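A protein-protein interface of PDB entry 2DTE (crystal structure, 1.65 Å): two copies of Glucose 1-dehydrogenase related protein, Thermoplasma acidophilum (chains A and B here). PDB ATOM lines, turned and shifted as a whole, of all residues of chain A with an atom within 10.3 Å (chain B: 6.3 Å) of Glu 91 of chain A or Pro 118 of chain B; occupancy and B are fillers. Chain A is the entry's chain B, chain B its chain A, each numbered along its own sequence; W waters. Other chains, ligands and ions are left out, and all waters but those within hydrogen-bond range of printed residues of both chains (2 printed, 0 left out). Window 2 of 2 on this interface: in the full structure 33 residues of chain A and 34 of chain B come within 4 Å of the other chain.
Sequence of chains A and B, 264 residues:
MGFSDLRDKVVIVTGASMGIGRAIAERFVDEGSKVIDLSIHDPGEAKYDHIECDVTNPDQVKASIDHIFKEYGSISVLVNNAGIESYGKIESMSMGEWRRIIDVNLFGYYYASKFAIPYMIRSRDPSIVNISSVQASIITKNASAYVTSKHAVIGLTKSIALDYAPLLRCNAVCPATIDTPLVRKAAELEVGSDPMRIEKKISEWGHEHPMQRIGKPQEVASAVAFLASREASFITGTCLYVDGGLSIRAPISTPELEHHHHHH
No position is printed for both chains. Of the 10 pairs that touch across the chains among the printed residues, none has its exchanged pair printed and touching as well.
Among the printed residues, merely in contact across the chains: Glu 91 of chain A with Tyr 164 of chain B (3.1 Å), Glu 91 of chain A with Pro 118 of chain B (3.2 Å), Ile 90 of chain A with Tyr 164 of chain B (3.5 Å), Lys 89 of chain A with Tyr 164 of chain B (3.5 Å), Met 95 of chain A with Lys 114 of chain B (3.6 Å), Ile 90 of chain A with Lys 114 of chain B (3.6 Å), Glu 91 of chain A with Ile 117 of chain B (3.6 Å), Ile 90 of chain A with Ile 117 of chain B (3.9 Å) and Met 95 of chain A with Phe 115 of chain B (3.97 Å).
O of Lys 114 of chain B lies close to OE2 of Glu 91 of chain A, at 2.5 Å.
The backbone NH (N) of Lys 89 of chain A lies within hydrogen-bond range of the side-chain hydroxyl (OG) of Ser 92 of chain A (3.1 Å). The side-chain amino group of Lys 89 of chain A lies within hydrogen-bond range of the side-chain amide oxygen of Asn 142 of chain A (2.6 Å).
Water W2 lies within hydrogen-bond range of the side-chain amino group of Lys 114 of chain B (2.6 Å), the backbone carbonyl oxygen of Met 93 of chain A (2.8 Å) and the backbone carbonyl oxygen of Glu 91 of chain A (3.2 Å). Water W1 lies within hydrogen-bond range of NZ of Lys 114 of chain B (2.6 Å) and OE1 of Glu 91 of chain A (2.7 Å).
Hydrophobic or aromatic side chains of chain B that line the printed part of chain A: Phe 115, Ile 117, Pro 118 and Tyr 164.
Tyr 87 of chain A touches none of the printed residues of chain B. Of the printed residues of chain B, Lys 89 of chain A touches Tyr 164. Printed residues of chain B within 4 Å of Ile 90 of chain A: Lys 114, Ile 117 and Tyr 164. Of the printed residues of chain A, Phe 115 of chain B touches Met 95. Of chain A, only Ile 90 (3.9 Å) and Glu 91 (3.6 Å) come within 4 Å of Ile 117 of chain B. Of the printed residues of chain A, Pro 118 of chain B touches Glu 91 (3.2 Å). Met 120 of chain B touches none of the printed residues of chain A. The nearest residue of chain B that does not touch Glu 91 of chain A is Ser 113 of chain B (4.1 Å). The nearest residue of chain A that does not touch Pro 118 of chain B is Ile 90 of chain A (7.0 Å). The nearest printed residue of chain B that does not touch Ile 90 of chain A is Ser 113 of chain B (4.1 Å).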
ATOM      1  N   TYR A  87       9.312 -12.207  11.212  1.00  0.00           N
ATOM      2  CA  TYR A  87       9.727 -12.335  12.600  1.00  0.00           C
ATOM      3  C   TYR A  87      10.898 -13.253  12.902  1.00  0.00           C
ATOM      4  O   TYR A  87      11.222 -14.166  12.134  1.00  0.00           O
ATOM      5  CB  TYR A  87       8.512 -12.770  13.431  1.00  0.00           C
ATOM      6  CG  TYR A  87       7.278 -11.943  13.138  1.00  0.00           C
ATOM      7  CD1 TYR A  87       6.985 -10.801  13.885  1.00  0.00           C
ATOM      8  CD2 TYR A  87       6.449 -12.256  12.062  1.00  0.00           C
ATOM      9  CE1 TYR A  87       5.903  -9.988  13.565  1.00  0.00           C
ATOM     10  CE2 TYR A  87       5.363 -11.449  11.726  1.00  0.00           C
ATOM     11  CZ  TYR A  87       5.097 -10.316  12.482  1.00  0.00           C
ATOM     12  OH  TYR A  87       4.038  -9.516  12.128  1.00  0.00           O
ATOM     13  N   GLY A  88      11.529 -12.993  14.040  1.00  0.00           N
ATOM     14  CA  GLY A  88      12.651 -13.801  14.476  1.00  0.00           C
ATOM     15  C   GLY A  88      13.580 -13.037  15.396  1.00  0.00           C
ATOM     16  O   GLY A  88      13.738 -11.823  15.261  1.00  0.00           O
ATOM     17  N   LYS A  89      14.177 -13.738  16.353  1.00  0.00           N
ATOM     18  CA  LYS A  89      15.107 -13.088  17.260  1.00  0.00           C
ATOM     19  C   LYS A  89      16.376 -12.834  16.466  1.00  0.00           C
ATOM     20  O   LYS A  89      16.610 -13.476  15.442  1.00  0.00           O
ATOM     21  CB  LYS A  89      15.395 -13.969  18.477  1.00  0.00           C
ATOM     22  CG  LYS A  89      14.233 -14.008  19.455  1.00  0.00           C
ATOM     23  CD  LYS A  89      14.619 -14.617  20.790  1.00  0.00           C
ATOM     24  CE  LYS A  89      13.448 -14.567  21.761  1.00  0.00           C
ATOM     25  NZ  LYS A  89      12.249 -15.263  21.220  1.00  0.00           N
ATOM     26  N   ILE A  90      17.182 -11.889  16.929  1.00  0.00           N
ATOM     27  CA  ILE A  90      18.411 -11.540  16.236  1.00  0.00           C
ATOM     28  C   ILE A  90      19.263 -12.775  15.934  1.00  0.00           C
ATOM     29  O   ILE A  90      20.067 -12.781  14.997  1.00  0.00           O
ATOM     30  CB  ILE A  90      19.213 -10.489  17.061  1.00  0.00           C
ATOM     31  CG1 ILE A  90      20.342  -9.909  16.212  1.00  0.00           C
ATOM     32  CG2 ILE A  90      19.755 -11.110  18.337  1.00  0.00           C
ATOM     33  CD1 ILE A  90      21.093  -8.780  16.898  1.00  0.00           C
ATOM     34  N   GLU A  91      19.053 -13.836  16.707  1.00  0.00           N
ATOM     35  CA  GLU A  91      19.803 -15.077  16.525  1.00  0.00           C
ATOM     36  C   GLU A  91      19.286 -16.021  15.442  1.00  0.00           C
ATOM     37  O   GLU A  91      20.069 -16.731  14.812  1.00  0.00           O
ATOM     38  CB  GLU A  91      19.862 -15.840  17.851  1.00  0.00           C
ATOM     39  CG  GLU A  91      20.710 -15.162  18.886  1.00  0.00           C
ATOM     40  CD  GLU A  91      22.055 -14.766  18.316  1.00  0.00           C
ATOM     41  OE1 GLU A  91      22.657 -15.597  17.601  1.00  0.00           O
ATOM     42  OE2 GLU A  91      22.506 -13.630  18.577  1.00  0.00           O
ATOM     43  N   SER A  92      17.976 -16.030  15.229  1.00  0.00           N
ATOM     44  CA  SER A  92      17.370 -16.928  14.251  1.00  0.00           C
ATOM     45  C   SER A  92      17.215 -16.360  12.846  1.00  0.00           C
ATOM     46  O   SER A  92      17.424 -17.070  11.858  1.00  0.00           O
ATOM     47  CB  SER A  92      16.002 -17.395  14.756  1.00  0.00           C
ATOM     48  OG  SER A  92      15.107 -16.302  14.876  1.00  0.00           O
ATOM     49  N   MET A  93      16.842 -15.091  12.743  1.00  0.00           N
ATOM     50  CA  MET A  93      16.667 -14.497  11.424  1.00  0.00           C
ATOM     51  C   MET A  93      18.009 -14.414  10.711  1.00  0.00           C
ATOM     52  O   MET A  93      19.019 -14.066  11.322  1.00  0.00           O
ATOM     53  CB  MET A  93      16.048 -13.103  11.545  1.00  0.00           C
ATOM     54  CG  MET A  93      15.699 -12.477  10.191  1.00  0.00           C
ATOM     55  SD  MET A  93      14.799 -10.903  10.332  1.00  0.00           S
ATOM     56  CE  MET A  93      13.157 -11.496  10.562  1.00  0.00           C
ATOM     57  N   SER A  94      18.023 -14.746   9.418  1.00  0.00           N
ATOM     58  CA  SER A  94      19.257 -14.682   8.642  1.00  0.00           C
ATOM     59  C   SER A  94      19.640 -13.218   8.495  1.00  0.00           C
ATOM     60  O   SER A  94      18.777 -12.334   8.559  1.00  0.00           O
ATOM     61  CB  SER A  94      19.061 -15.283   7.246  1.00  0.00           C
ATOM     62  OG  SER A  94      18.198 -14.477   6.456  1.00  0.00           O
ATOM     63  N   MET A  95      20.926 -12.959   8.307  1.00  0.00           N
ATOM     64  CA  MET A  95      21.377 -11.586   8.141  1.00  0.00           C
ATOM     65  C   MET A  95      20.754 -11.019   6.870  1.00  0.00           C
ATOM     66  O   MET A  95      20.403  -9.845   6.814  1.00  0.00           O
ATOM     67  CB  MET A  95      22.906 -11.524   8.067  1.00  0.00           C
ATOM     68  CG  MET A  95      23.599 -11.943   9.368  1.00  0.00           C
ATOM     69  SD  MET A  95      25.341 -11.530   9.411  1.00  0.00           S
ATOM     70  CE  MET A  95      26.008 -12.720   8.161  1.00  0.00           C
ATOM     71  N   GLY A  96      20.606 -11.858   5.851  1.00  0.00           N
ATOM     72  CA  GLY A  96      20.016 -11.382   4.616  1.00  0.00           C
ATOM     73  C   GLY A  96      18.594 -10.882   4.797  1.00  0.00           C
ATOM     74  O   GLY A  96      18.218  -9.853   4.225  1.00  0.00           O
ATOM     75  N   TRP A  98      17.279  -9.863   7.627  1.00  0.00           N
ATOM     76  CA  TRP A  98      17.327  -8.704   8.522  1.00  0.00           C
ATOM     77  C   TRP A  98      17.638  -7.460   7.679  1.00  0.00           C
ATOM     78  O   TRP A  98      16.964  -6.430   7.795  1.00  0.00           O
ATOM     79  CB  TRP A  98      18.405  -8.917   9.600  1.00  0.00           C
ATOM     80  CG  TRP A  98      18.164  -8.173  10.896  1.00  0.00           C
ATOM     81  CD1 TRP A  98      17.508  -8.643  12.004  1.00  0.00           C
ATOM     82  CD2 TRP A  98      18.588  -6.840  11.215  1.00  0.00           C
ATOM     83  NE1 TRP A  98      17.500  -7.683  12.995  1.00  0.00           N
ATOM     84  CE2 TRP A  98      18.155  -6.567  12.539  1.00  0.00           C
ATOM     85  CE3 TRP A  98      19.295  -5.848  10.514  1.00  0.00           C
ATOM     86  CZ2 TRP A  98      18.409  -5.337  13.176  1.00  0.00           C
ATOM     87  CZ3 TRP A  98      19.549  -4.626  11.151  1.00  0.00           C
ATOM     88  CH2 TRP A  98      19.103  -4.389  12.469  1.00  0.00           C
ATOM     89  N   ASN A 142      10.515 -10.498  19.075  1.00  0.00           N
ATOM     90  CA  ASN A 142      10.919 -11.184  17.847  1.00  0.00           C
ATOM     91  C   ASN A 142      10.714 -10.347  16.603  1.00  0.00           C
ATOM     92  O   ASN A 142      10.381 -10.880  15.544  1.00  0.00           O
ATOM     93  CB  ASN A 142      10.147 -12.502  17.698  1.00  0.00           C
ATOM     94  CG  ASN A 142      10.235 -13.366  18.935  1.00  0.00           C
ATOM     95  OD1 ASN A 142      11.302 -13.514  19.526  1.00  0.00           O
ATOM     96  ND2 ASN A 142       9.107 -13.949  19.330  1.00  0.00           N
ATOM     97  N   ALA A 143      10.930  -9.040  16.731  1.00  0.00           N
ATOM     98  CA  ALA A 143      10.750  -8.130  15.605  1.00  0.00           C
ATOM     99  C   ALA A 143      11.896  -7.127  15.501  1.00  0.00           C
ATOM    100  O   ALA A 143      11.685  -5.977  15.108  1.00  0.00           O
ATOM    101  CB  ALA A 143       9.411  -7.400  15.745  1.00  0.00           C
ATOM    102  N   SER A 144      13.107  -7.585  15.829  1.00  0.00           N
ATOM    103  CA  SER A 144      14.321  -6.769  15.804  1.00  0.00           C
ATOM    104  C   SER A 144      14.471  -5.871  14.568  1.00  0.00           C
ATOM    105  O   SER A 144      14.588  -4.647  14.681  1.00  0.00           O
ATOM    106  CB  SER A 144      15.556  -7.680  15.908  1.00  0.00           C
ATOM    107  OG  SER A 144      16.746  -6.923  15.803  1.00  0.00           O
ATOM    108  N   ALA A 145      14.475  -6.469  13.380  1.00  0.00           N
ATOM    109  CA  ALA A 145      14.649  -5.672  12.164  1.00  0.00           C
ATOM    110  C   ALA A 145      13.527  -4.671  11.947  1.00  0.00           C
ATOM    111  O   ALA A 145      13.762  -3.504  11.588  1.00  0.00           O
ATOM    112  CB  ALA A 145      14.747  -6.592  10.945  1.00  0.00           C
ATOM    113  N   SER B 113      26.331  -7.595  18.305  1.00  0.00           N
ATOM    114  CA  SER B 113      25.324  -8.138  19.210  1.00  0.00           C
ATOM    115  C   SER B 113      24.927  -9.540  18.814  1.00  0.00           C
ATOM    116  O   SER B 113      24.876 -10.436  19.653  1.00  0.00           O
ATOM    117  CB  SER B 113      24.065  -7.256  19.225  1.00  0.00           C
ATOM    118  OG  SER B 113      24.393  -5.961  19.685  1.00  0.00           O
ATOM    119  N   LYS B 114      24.660  -9.736  17.526  1.00  0.00           N
ATOM    120  CA  LYS B 114      24.230 -11.037  17.047  1.00  0.00           C
ATOM    121  C   LYS B 114      25.222 -12.156  17.355  1.00  0.00           C
ATOM    122  O   LYS B 114      24.815 -13.260  17.725  1.00  0.00           O
ATOM    123  CB  LYS B 114      23.975 -10.979  15.537  1.00  0.00           C
ATOM    124  CG  LYS B 114      23.625 -12.319  14.905  1.00  0.00           C
ATOM    125  CD  LYS B 114      23.242 -12.138  13.436  1.00  0.00           C
ATOM    126  CE  LYS B 114      23.569 -13.375  12.630  1.00  0.00           C
ATOM    127  NZ  LYS B 114      22.942 -14.605  13.143  1.00  0.00           N
ATOM    128  N   PHE B 115      26.510 -11.874  17.224  1.00  0.00           N
ATOM    129  CA  PHE B 115      27.508 -12.913  17.465  1.00  0.00           C
ATOM    130  C   PHE B 115      27.951 -13.047  18.909  1.00  0.00           C
ATOM    131  O   PHE B 115      28.427 -14.106  19.309  1.00  0.00           O
ATOM    132  CB  PHE B 115      28.701 -12.709  16.524  1.00  0.00           C
ATOM    133  CG  PHE B 115      28.328 -12.852  15.079  1.00  0.00           C
ATOM    134  CD1 PHE B 115      28.437 -11.778  14.198  1.00  0.00           C
ATOM    135  CD2 PHE B 115      27.753 -14.037  14.625  1.00  0.00           C
ATOM    136  CE1 PHE B 115      27.964 -11.883  12.884  1.00  0.00           C
ATOM    137  CE2 PHE B 115      27.280 -14.156  13.325  1.00  0.00           C
ATOM    138  CZ  PHE B 115      27.383 -13.072  12.446  1.00  0.00           C
ATOM    139  N   ALA B 116      27.774 -11.998  19.709  1.00  0.00           N
ATOM    140  CA  ALA B 116      28.175 -12.085  21.109  1.00  0.00           C
ATOM    141  C   ALA B 116      27.099 -12.716  21.984  1.00  0.00           C
ATOM    142  O   ALA B 116      27.411 -13.454  22.925  1.00  0.00           O
ATOM    143  CB  ALA B 116      28.517 -10.699  21.648  1.00  0.00           C
ATOM    144  N   ILE B 117      25.838 -12.438  21.669  1.00  0.00           N
ATOM    145  CA  ILE B 117      24.734 -12.931  22.486  1.00  0.00           C
ATOM    146  C   ILE B 117      24.741 -14.417  22.850  1.00  0.00           C
ATOM    147  O   ILE B 117      24.604 -14.754  24.025  1.00  0.00           O
ATOM    148  CB  ILE B 117      23.367 -12.495  21.878  1.00  0.00           C
ATOM    149  CG1 ILE B 117      23.161 -10.998  22.147  1.00  0.00           C
ATOM    150  CG2 ILE B 117      22.210 -13.284  22.498  1.00  0.00           C
ATOM    151  CD1 ILE B 117      21.986 -10.369  21.404  1.00  0.00           C
ATOM    152  N   PRO B 118      24.942 -15.318  21.874  1.00  0.00           N
ATOM    153  CA  PRO B 118      24.944 -16.752  22.213  1.00  0.00           C
ATOM    154  C   PRO B 118      25.934 -17.089  23.328  1.00  0.00           C
ATOM    155  O   PRO B 118      25.655 -17.929  24.190  1.00  0.00           O
ATOM    156  CB  PRO B 118      25.302 -17.421  20.886  1.00  0.00           C
ATOM    157  CG  PRO B 118      24.720 -16.453  19.861  1.00  0.00           C
ATOM    158  CD  PRO B 118      25.137 -15.111  20.428  1.00  0.00           C
ATOM    159  N   TYR B 119      27.088 -16.433  23.303  1.00  0.00           N
ATOM    160  CA  TYR B 119      28.116 -16.635  24.318  1.00  0.00           C
ATOM    161  C   TYR B 119      27.745 -15.944  25.624  1.00  0.00           C
ATOM    162  O   TYR B 119      27.922 -16.488  26.706  1.00  0.00           O
ATOM    163  CB  TYR B 119      29.440 -16.071  23.835  1.00  0.00           C
ATOM    164  CG  TYR B 119      30.016 -16.804  22.646  1.00  0.00           C
ATOM    165  CD1 TYR B 119      30.301 -16.133  21.460  1.00  0.00           C
ATOM    166  CD2 TYR B 119      30.333 -18.162  22.726  1.00  0.00           C
ATOM    167  CE1 TYR B 119      30.898 -16.791  20.383  1.00  0.00           C
ATOM    168  CE2 TYR B 119      30.927 -18.825  21.657  1.00  0.00           C
ATOM    169  CZ  TYR B 119      31.212 -18.136  20.494  1.00  0.00           C
ATOM    170  OH  TYR B 119      31.862 -18.776  19.458  1.00  0.00           O
ATOM    171  N   MET B 120      27.236 -14.722  25.515  1.00  0.00           N
ATOM    172  CA  MET B 120      26.866 -13.960  26.696  1.00  0.00           C
ATOM    173  C   MET B 120      25.813 -14.636  27.573  1.00  0.00           C
ATOM    174  O   MET B 120      25.888 -14.560  28.805  1.00  0.00           O
ATOM    175  CB  MET B 120      26.393 -12.569  26.266  1.00  0.00           C
ATOM    176  CG  MET B 120      27.519 -11.729  25.709  1.00  0.00           C
ATOM    177  SD  MET B 120      26.984 -10.105  25.094  1.00  0.00           S
ATOM    178  CE  MET B 120      26.705  -9.231  26.674  1.00  0.00           C
ATOM    179  N   ILE B 121      24.831 -15.283  26.953  1.00  0.00           N
ATOM    180  CA  ILE B 121      23.796 -15.950  27.722  1.00  0.00           C
ATOM    181  C   ILE B 121      24.344 -17.164  28.471  1.00  0.00           C
ATOM    182  O   ILE B 121      23.633 -17.769  29.268  1.00  0.00           O
ATOM    183  CB  ILE B 121      22.592 -16.370  26.847  1.00  0.00           C
ATOM    184  CG1 ILE B 121      23.042 -17.271  25.698  1.00  0.00           C
ATOM    185  CG2 ILE B 121      21.887 -15.121  26.315  1.00  0.00           C
ATOM    186  CD1 ILE B 121      21.884 -17.757  24.838  1.00  0.00           C
ATOM    187  N   ARG B 122      25.604 -17.512  28.214  1.00  0.00           N
ATOM    188  CA  ARG B 122      26.238 -18.627  28.916  1.00  0.00           C
ATOM    189  C   ARG B 122      26.916 -18.102  30.182  1.00  0.00           C
ATOM    190  O   ARG B 122      27.505 -18.869  30.952  1.00  0.00           O
ATOM    191  CB  ARG B 122      27.275 -19.320  28.036  1.00  0.00           C
ATOM    192  CG  ARG B 122      26.697 -20.009  26.821  1.00  0.00           C
ATOM    193  CD  ARG B 122      27.800 -20.675  26.024  1.00  0.00           C
ATOM    194  NE  ARG B 122      27.397 -20.936  24.648  1.00  0.00           N
ATOM    195  CZ  ARG B 122      28.218 -21.389  23.704  1.00  0.00           C
ATOM    196  NH1 ARG B 122      29.491 -21.637  23.994  1.00  0.00           N
ATOM    197  NH2 ARG B 122      27.771 -21.572  22.466  1.00  0.00           N
ATOM    198  N   TYR B 164      15.591 -10.795  24.960  1.00  0.00           N
ATOM    199  CA  TYR B 164      16.410 -11.607  25.854  1.00  0.00           C
ATOM    200  C   TYR B 164      16.228 -11.437  27.367  1.00  0.00           C
ATOM    201  O   TYR B 164      16.944 -12.065  28.161  1.00  0.00           O
ATOM    202  CB  TYR B 164      17.881 -11.458  25.451  1.00  0.00           C
ATOM    203  CG  TYR B 164      18.127 -12.011  24.064  1.00  0.00           C
ATOM    204  CD1 TYR B 164      18.025 -11.200  22.933  1.00  0.00           C
ATOM    205  CD2 TYR B 164      18.349 -13.372  23.875  1.00  0.00           C
ATOM    206  CE1 TYR B 164      18.131 -11.739  21.649  1.00  0.00           C
ATOM    207  CE2 TYR B 164      18.452 -13.919  22.605  1.00  0.00           C
ATOM    208  CZ  TYR B 164      18.339 -13.101  21.495  1.00  0.00           C
ATOM    209  OH  TYR B 164      18.399 -13.668  20.237  1.00  0.00           O
HETATM  210  O   HOH W   1      24.146 -15.290  15.315  1.00  0.00           O
HETATM  211  O   HOH W   2      21.091 -15.894  11.916  1.00  0.00           O
